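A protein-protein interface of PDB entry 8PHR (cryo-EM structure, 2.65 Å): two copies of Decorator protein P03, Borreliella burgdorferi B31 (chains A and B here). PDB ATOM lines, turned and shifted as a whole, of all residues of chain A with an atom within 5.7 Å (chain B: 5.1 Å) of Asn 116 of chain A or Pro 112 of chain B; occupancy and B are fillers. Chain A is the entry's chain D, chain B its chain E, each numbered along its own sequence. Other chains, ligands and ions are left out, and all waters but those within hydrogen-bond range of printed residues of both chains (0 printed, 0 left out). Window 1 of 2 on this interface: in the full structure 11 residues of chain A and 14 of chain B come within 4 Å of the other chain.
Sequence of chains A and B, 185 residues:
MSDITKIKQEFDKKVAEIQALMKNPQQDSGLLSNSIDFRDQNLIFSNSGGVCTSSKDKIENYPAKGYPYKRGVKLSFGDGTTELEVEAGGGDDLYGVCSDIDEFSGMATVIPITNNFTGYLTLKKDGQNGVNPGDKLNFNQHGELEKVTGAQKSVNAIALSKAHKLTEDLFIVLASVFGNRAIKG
The side-chain carboxylate (OE2) of Glu 60 of chain B is in hydrogen-bond range of the side-chain amide nitrogen (ND2) of Asn 116 of chain A, 3.1 Å away.
The side-chain amino group (NZ) of Lys 58 of chain B is in salt-bridge range of the side-chain carboxylate (OD1) of Asp 57 of chain A (3.0 Å).
Of the 11 printed residues of chain B, 4 touch a printed residue of chain A.
Hydrophobic or aromatic side chains of chain B within 4 Å of the printed part of chain A: Pro 112.
Among the printed residues, 6 pairs touch across the chains.
Among the printed residues, Asp or Glu carboxylates within 4 Å of a Lys or Arg side-chain nitrogen of the other chain: Asp 57 of chain A with Lys 58 of chain B (3.0 Å).
Thr 114 of chain A touches Thr 114 of chain B.
Asn 116 of chain A touches Lys 58 of chain B (OD1 to CE, 3.1 Å).
Asn 116 of chain A touches Pro 112 of chain B (ND2 to CG, 3.3 Å).
N of Asn 116 of chain A touches OG1 of Thr 114 of chain B, 3.8 Å away.
Pro 112 of chain B touches just one residue of chain A: Asn 116.
Of the printed residues of chain B, Thr 114 of chain A touches Thr 114.
Of the printed residues of chain B, Asp 57 of chain A touches Lys 58.
Printed residues of chain A within 4 Å of Thr 114 of chain B: Thr 114 and Asn 116.
Printed residues of chain A within 4 Å of Lys 58 of chain B: Asp 57 and Asn 116.
Of the printed residues of chain A, Glu 60 of chain B touches Asn 116.
Ile 111 of chain A touches none of the printed residues of chain B.
The nearest printed residue of chain A that does not touch Pro 112 of chain B is Phe 178 of chain A (6.9 Å).
The side-chain amide nitrogen (ND2) of Asn 115 of chain B sits close to the backbone NH (N) of Lys 58 of chain B (3.1 Å).
The side-chain amide oxygen of Asn 116 of chain A sits close to the side-chain amide oxygen of Asn 115 of chain A (3.2 Å).
The backbone NH (N) of Val 110 of chain B sits at hydrogen-bond distance from the backbone carbonyl oxygen (O) of Glu 60 of chain B (2.9 Å).
OH of Tyr 95 of chain B lies within hydrogen-bond range of OE1 of Glu 60 of chain B (3.0 Å).
Thr 114 of chain A touches its own counterpart, Thr 114 of chain B.
5 positions are printed for both chains.
Of the 6 pairs that touch across the chains among the printed residues, 1 has its exchanged pair printed and touching as well.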
ATOM      1  N   ASP A  57      -4.450  28.889   0.721  1.00  0.00           N
ATOM      2  CA  ASP A  57      -4.342  29.623  -0.532  1.00  0.00           C
ATOM      3  C   ASP A  57      -4.902  31.029  -0.370  1.00  0.00           C
ATOM      4  O   ASP A  57      -5.931  31.232   0.281  1.00  0.00           O
ATOM      5  CB  ASP A  57      -5.082  28.892  -1.653  1.00  0.00           C
ATOM      6  CG  ASP A  57      -4.483  27.533  -1.957  1.00  0.00           C
ATOM      7  OD1 ASP A  57      -3.492  27.157  -1.296  1.00  0.00           O
ATOM      8  OD2 ASP A  57      -5.003  26.840  -2.857  1.00  0.00           O
ATOM      9  N   ILE A 111      -6.155  34.466  -7.881  1.00  0.00           N
ATOM     10  CA  ILE A 111      -5.035  33.929  -7.118  1.00  0.00           C
ATOM     11  C   ILE A 111      -3.776  34.654  -7.581  1.00  0.00           C
ATOM     12  O   ILE A 111      -3.484  34.647  -8.788  1.00  0.00           O
ATOM     13  CB  ILE A 111      -4.898  32.411  -7.306  1.00  0.00           C
ATOM     14  CG1 ILE A 111      -6.149  31.699  -6.788  1.00  0.00           C
ATOM     15  CG2 ILE A 111      -3.651  31.899  -6.599  1.00  0.00           C
ATOM     16  CD1 ILE A 111      -6.022  30.193  -6.735  1.00  0.00           C
ATOM     17  N   PRO A 112      -3.033  35.302  -6.688  1.00  0.00           N
ATOM     18  CA  PRO A 112      -1.847  36.051  -7.113  1.00  0.00           C
ATOM     19  C   PRO A 112      -0.778  35.137  -7.691  1.00  0.00           C
ATOM     20  O   PRO A 112      -0.716  33.939  -7.406  1.00  0.00           O
ATOM     21  CB  PRO A 112      -1.361  36.719  -5.820  1.00  0.00           C
ATOM     22  CG  PRO A 112      -2.554  36.730  -4.921  1.00  0.00           C
ATOM     23  CD  PRO A 112      -3.321  35.487  -5.256  1.00  0.00           C
ATOM     24  N   ILE A 113       0.072  35.735  -8.532  1.00  0.00           N
ATOM     25  CA  ILE A 113       1.166  34.989  -9.148  1.00  0.00           C
ATOM     26  C   ILE A 113       2.123  34.461  -8.087  1.00  0.00           C
ATOM     27  O   ILE A 113       2.823  33.464  -8.309  1.00  0.00           O
ATOM     28  CB  ILE A 113       1.889  35.870 -10.187  1.00  0.00           C
ATOM     29  CG1 ILE A 113       2.854  35.033 -11.029  1.00  0.00           C
ATOM     30  CG2 ILE A 113       2.622  37.018  -9.507  1.00  0.00           C
ATOM     31  CD1 ILE A 113       2.169  33.978 -11.868  1.00  0.00           C
ATOM     32  N   THR A 114       2.170  35.110  -6.920  1.00  0.00           N
ATOM     33  CA  THR A 114       3.000  34.624  -5.823  1.00  0.00           C
ATOM     34  C   THR A 114       2.514  33.290  -5.274  1.00  0.00           C
ATOM     35  O   THR A 114       3.279  32.600  -4.592  1.00  0.00           O
ATOM     36  CB  THR A 114       3.038  35.654  -4.692  1.00  0.00           C
ATOM     37  OG1 THR A 114       1.728  35.796  -4.128  1.00  0.00           O
ATOM     38  CG2 THR A 114       3.510  37.001  -5.211  1.00  0.00           C
ATOM     39  N   ASN A 115       1.269  32.914  -5.551  1.00  0.00           N
ATOM     40  CA  ASN A 115       0.703  31.653  -5.101  1.00  0.00           C
ATOM     41  C   ASN A 115       0.503  30.730  -6.295  1.00  0.00           C
ATOM     42  O   ASN A 115      -0.003  31.152  -7.340  1.00  0.00           O
ATOM     43  CB  ASN A 115      -0.629  31.880  -4.380  1.00  0.00           C
ATOM     44  CG  ASN A 115      -1.000  30.731  -3.463  1.00  0.00           C
ATOM     45  OD1 ASN A 115      -1.115  29.586  -3.899  1.00  0.00           O
ATOM     46  ND2 ASN A 115      -1.190  31.033  -2.184  1.00  0.00           N
ATOM     47  N   ASN A 116       0.905  29.473  -6.137  1.00  0.00           N
ATOM     48  CA  ASN A 116       0.760  28.504  -7.209  1.00  0.00           C
ATOM     49  C   ASN A 116      -0.693  28.050  -7.337  1.00  0.00           C
ATOM     50  O   ASN A 116      -1.481  28.114  -6.389  1.00  0.00           O
ATOM     51  CB  ASN A 116       1.679  27.303  -6.976  1.00  0.00           C
ATOM     52  CG  ASN A 116       1.347  26.544  -5.706  1.00  0.00           C
ATOM     53  OD1 ASN A 116       0.538  26.991  -4.895  1.00  0.00           O
ATOM     54  ND2 ASN A 116       1.969  25.384  -5.533  1.00  0.00           N
ATOM     55  N   PHE A 117      -1.044  27.596  -8.538  1.00  0.00           N
ATOM     56  CA  PHE A 117      -2.402  27.166  -8.829  1.00  0.00           C
ATOM     57  C   PHE A 117      -2.368  25.984  -9.785  1.00  0.00           C
ATOM     58  O   PHE A 117      -1.512  25.918 -10.672  1.00  0.00           O
ATOM     59  CB  PHE A 117      -3.231  28.310  -9.432  1.00  0.00           C
ATOM     60  CG  PHE A 117      -4.558  27.874  -9.985  1.00  0.00           C
ATOM     61  CD1 PHE A 117      -5.589  27.507  -9.136  1.00  0.00           C
ATOM     62  CD2 PHE A 117      -4.776  27.831 -11.353  1.00  0.00           C
ATOM     63  CE1 PHE A 117      -6.813  27.107  -9.640  1.00  0.00           C
ATOM     64  CE2 PHE A 117      -5.997  27.430 -11.862  1.00  0.00           C
ATOM     65  CZ  PHE A 117      -7.017  27.068 -11.005  1.00  0.00           C
ATOM     66  N   THR A 118      -3.301  25.053  -9.596  1.00  0.00           N
ATOM     67  CA  THR A 118      -3.442  23.883 -10.458  1.00  0.00           C
ATOM     68  C   THR A 118      -4.908  23.759 -10.849  1.00  0.00           C
ATOM     69  O   THR A 118      -5.766  23.532  -9.990  1.00  0.00           O
ATOM     70  CB  THR A 118      -2.954  22.613  -9.759  1.00  0.00           C
ATOM     71  OG1 THR A 118      -1.652  22.840  -9.207  1.00  0.00           O
ATOM     72  CG2 THR A 118      -2.888  21.454 -10.744  1.00  0.00           C
ATOM     73  N   VAL A 177       0.716  26.360 -12.456  1.00  0.00           N
ATOM     74  CA  VAL A 177       1.383  27.657 -12.480  1.00  0.00           C
ATOM     75  C   VAL A 177       2.336  27.743 -11.296  1.00  0.00           C
ATOM     76  O   VAL A 177       1.952  27.452 -10.157  1.00  0.00           O
ATOM     77  CB  VAL A 177       0.359  28.803 -12.449  1.00  0.00           C
ATOM     78  CG1 VAL A 177       1.042  30.132 -12.723  1.00  0.00           C
ATOM     79  CG2 VAL A 177      -0.752  28.548 -13.456  1.00  0.00           C
ATOM     80  N   PHE A 178       3.579  28.136 -11.563  1.00  0.00           N
ATOM     81  CA  PHE A 178       4.610  28.250 -10.539  1.00  0.00           C
ATOM     82  C   PHE A 178       5.303  29.604 -10.605  1.00  0.00           C
ATOM     83  O   PHE A 178       6.506  29.722 -10.357  1.00  0.00           O
ATOM     84  CB  PHE A 178       5.618  27.104 -10.646  1.00  0.00           C
ATOM     85  CG  PHE A 178       6.254  26.970 -12.003  1.00  0.00           C
ATOM     86  CD1 PHE A 178       5.668  26.179 -12.976  1.00  0.00           C
ATOM     87  CD2 PHE A 178       7.445  27.613 -12.299  1.00  0.00           C
ATOM     88  CE1 PHE A 178       6.246  26.043 -14.224  1.00  0.00           C
ATOM     89  CE2 PHE A 178       8.030  27.481 -13.546  1.00  0.00           C
ATOM     90  CZ  PHE A 178       7.430  26.694 -14.509  1.00  0.00           C
ATOM     91  N   LYS B  58       1.955  26.093   2.542  1.00  0.00           N
ATOM     92  CA  LYS B  58       1.298  25.182   1.614  1.00  0.00           C
ATOM     93  C   LYS B  58       2.160  23.937   1.443  1.00  0.00           C
ATOM     94  O   LYS B  58       3.341  24.038   1.093  1.00  0.00           O
ATOM     95  CB  LYS B  58       1.054  25.856   0.266  1.00  0.00           C
ATOM     96  CG  LYS B  58       0.120  25.078  -0.648  1.00  0.00           C
ATOM     97  CD  LYS B  58      -0.071  25.788  -1.976  1.00  0.00           C
ATOM     98  CE  LYS B  58      -0.783  24.898  -2.983  1.00  0.00           C
ATOM     99  NZ  LYS B  58      -2.246  24.822  -2.734  1.00  0.00           N
ATOM    100  N   ILE B  59       1.570  22.771   1.689  1.00  0.00           N
ATOM    101  CA  ILE B  59       2.271  21.492   1.641  1.00  0.00           C
ATOM    102  C   ILE B  59       1.518  20.563   0.700  1.00  0.00           C
ATOM    103  O   ILE B  59       0.301  20.390   0.838  1.00  0.00           O
ATOM    104  CB  ILE B  59       2.395  20.868   3.042  1.00  0.00           C
ATOM    105  CG1 ILE B  59       3.145  21.813   3.985  1.00  0.00           C
ATOM    106  CG2 ILE B  59       3.076  19.519   2.969  1.00  0.00           C
ATOM    107  CD1 ILE B  59       3.168  21.348   5.423  1.00  0.00           C
ATOM    108  N   GLU B  60       2.234  19.971  -0.253  1.00  0.00           N
ATOM    109  CA  GLU B  60       1.654  19.033  -1.202  1.00  0.00           C
ATOM    110  C   GLU B  60       2.309  17.667  -1.034  1.00  0.00           C
ATOM    111  O   GLU B  60       3.344  17.526  -0.380  1.00  0.00           O
ATOM    112  CB  GLU B  60       1.825  19.534  -2.641  1.00  0.00           C
ATOM    113  CG  GLU B  60       1.173  20.881  -2.905  1.00  0.00           C
ATOM    114  CD  GLU B  60       1.639  21.512  -4.202  1.00  0.00           C
ATOM    115  OE1 GLU B  60       2.555  20.955  -4.842  1.00  0.00           O
ATOM    116  OE2 GLU B  60       1.090  22.568  -4.581  1.00  0.00           O
ATOM    117  N   TYR B  95      10.576  22.569  -9.402  1.00  0.00           N
ATOM    118  CA  TYR B  95       9.202  22.784  -8.970  1.00  0.00           C
ATOM    119  C   TYR B  95       9.082  23.075  -7.482  1.00  0.00           C
ATOM    120  O   TYR B  95       8.178  23.814  -7.078  1.00  0.00           O
ATOM    121  CB  TYR B  95       8.344  21.561  -9.315  1.00  0.00           C
ATOM    122  CG  TYR B  95       6.905  21.669  -8.864  1.00  0.00           C
ATOM    123  CD1 TYR B  95       6.022  22.535  -9.494  1.00  0.00           C
ATOM    124  CD2 TYR B  95       6.429  20.903  -7.807  1.00  0.00           C
ATOM    125  CE1 TYR B  95       4.706  22.637  -9.086  1.00  0.00           C
ATOM    126  CE2 TYR B  95       5.114  20.998  -7.391  1.00  0.00           C
ATOM    127  CZ  TYR B  95       4.258  21.866  -8.034  1.00  0.00           C
ATOM    128  OH  TYR B  95       2.948  21.964  -7.622  1.00  0.00           O
ATOM    129  N   GLY B  96       9.967  22.521  -6.665  1.00  0.00           N
ATOM    130  CA  GLY B  96       9.904  22.759  -5.237  1.00  0.00           C
ATOM    131  C   GLY B  96      11.027  22.049  -4.519  1.00  0.00           C
ATOM    132  O   GLY B  96      12.026  21.661  -5.130  1.00  0.00           O
ATOM    133  N   VAL B 110       6.171  17.915  -0.607  1.00  0.00           N
ATOM    134  CA  VAL B 110       6.777  18.975  -1.399  1.00  0.00           C
ATOM    135  C   VAL B 110       6.290  20.324  -0.887  1.00  0.00           C
ATOM    136  O   VAL B 110       5.095  20.514  -0.631  1.00  0.00           O
ATOM    137  CB  VAL B 110       6.454  18.811  -2.901  1.00  0.00           C
ATOM    138  CG1 VAL B 110       6.935  20.019  -3.692  1.00  0.00           C
ATOM    139  CG2 VAL B 110       7.079  17.532  -3.441  1.00  0.00           C
ATOM    140  N   ILE B 111       7.226  21.249  -0.725  1.00  0.00           N
ATOM    141  CA  ILE B 111       6.945  22.656  -0.460  1.00  0.00           C
ATOM    142  C   ILE B 111       7.230  23.426  -1.744  1.00  0.00           C
ATOM    143  O   ILE B 111       8.376  23.429  -2.212  1.00  0.00           O
ATOM    144  CB  ILE B 111       7.783  23.195   0.710  1.00  0.00           C
ATOM    145  CG1 ILE B 111       7.398  22.483   2.009  1.00  0.00           C
ATOM    146  CG2 ILE B 111       7.604  24.699   0.845  1.00  0.00           C
ATOM    147  CD1 ILE B 111       8.096  23.024   3.236  1.00  0.00           C
ATOM    148  N   PRO B 112       6.235  24.072  -2.350  1.00  0.00           N
ATOM    149  CA  PRO B 112       6.443  24.692  -3.663  1.00  0.00           C
ATOM    150  C   PRO B 112       7.462  25.819  -3.608  1.00  0.00           C
ATOM    151  O   PRO B 112       7.705  26.431  -2.565  1.00  0.00           O
ATOM    152  CB  PRO B 112       5.050  25.220  -4.033  1.00  0.00           C
ATOM    153  CG  PRO B 112       4.102  24.431  -3.182  1.00  0.00           C
ATOM    154  CD  PRO B 112       4.836  24.178  -1.904  1.00  0.00           C
ATOM    155  N   ILE B 113       8.071  26.084  -4.768  1.00  0.00           N
ATOM    156  CA  ILE B 113       9.071  27.140  -4.873  1.00  0.00           C
ATOM    157  C   ILE B 113       8.471  28.511  -4.587  1.00  0.00           C
ATOM    158  O   ILE B 113       9.203  29.447  -4.245  1.00  0.00           O
ATOM    159  CB  ILE B 113       9.732  27.102  -6.266  1.00  0.00           C
ATOM    160  CG1 ILE B 113      11.023  27.924  -6.279  1.00  0.00           C
ATOM    161  CG2 ILE B 113       8.767  27.599  -7.335  1.00  0.00           C
ATOM    162  CD1 ILE B 113      12.052  27.459  -5.274  1.00  0.00           C
ATOM    163  N   THR B 114       7.150  28.653  -4.701  1.00  0.00           N
ATOM    164  CA  THR B 114       6.482  29.906  -4.380  1.00  0.00           C
ATOM    165  C   THR B 114       6.334  30.128  -2.881  1.00  0.00           C
ATOM    166  O   THR B 114       5.915  31.217  -2.473  1.00  0.00           O
ATOM    167  CB  THR B 114       5.101  29.952  -5.040  1.00  0.00           C
ATOM    168  OG1 THR B 114       4.246  28.977  -4.430  1.00  0.00           O
ATOM    169  CG2 THR B 114       5.213  29.659  -6.528  1.00  0.00           C
ATOM    170  N   ASN B 115       6.666  29.137  -2.062  1.00  0.00           N
ATOM    171  CA  ASN B 115       6.573  29.236  -0.613  1.00  0.00           C
ATOM    172  C   ASN B 115       7.970  29.263  -0.011  1.00  0.00           C
ATOM    173  O   ASN B 115       8.868  28.546  -0.466  1.00  0.00           O
ATOM    174  CB  ASN B 115       5.773  28.065  -0.034  1.00  0.00           C
ATOM    175  CG  ASN B 115       5.289  28.329   1.378  1.00  0.00           C
ATOM    176  OD1 ASN B 115       6.080  28.613   2.277  1.00  0.00           O
ATOM    177  ND2 ASN B 115       3.980  28.237   1.581  1.00  0.00           N
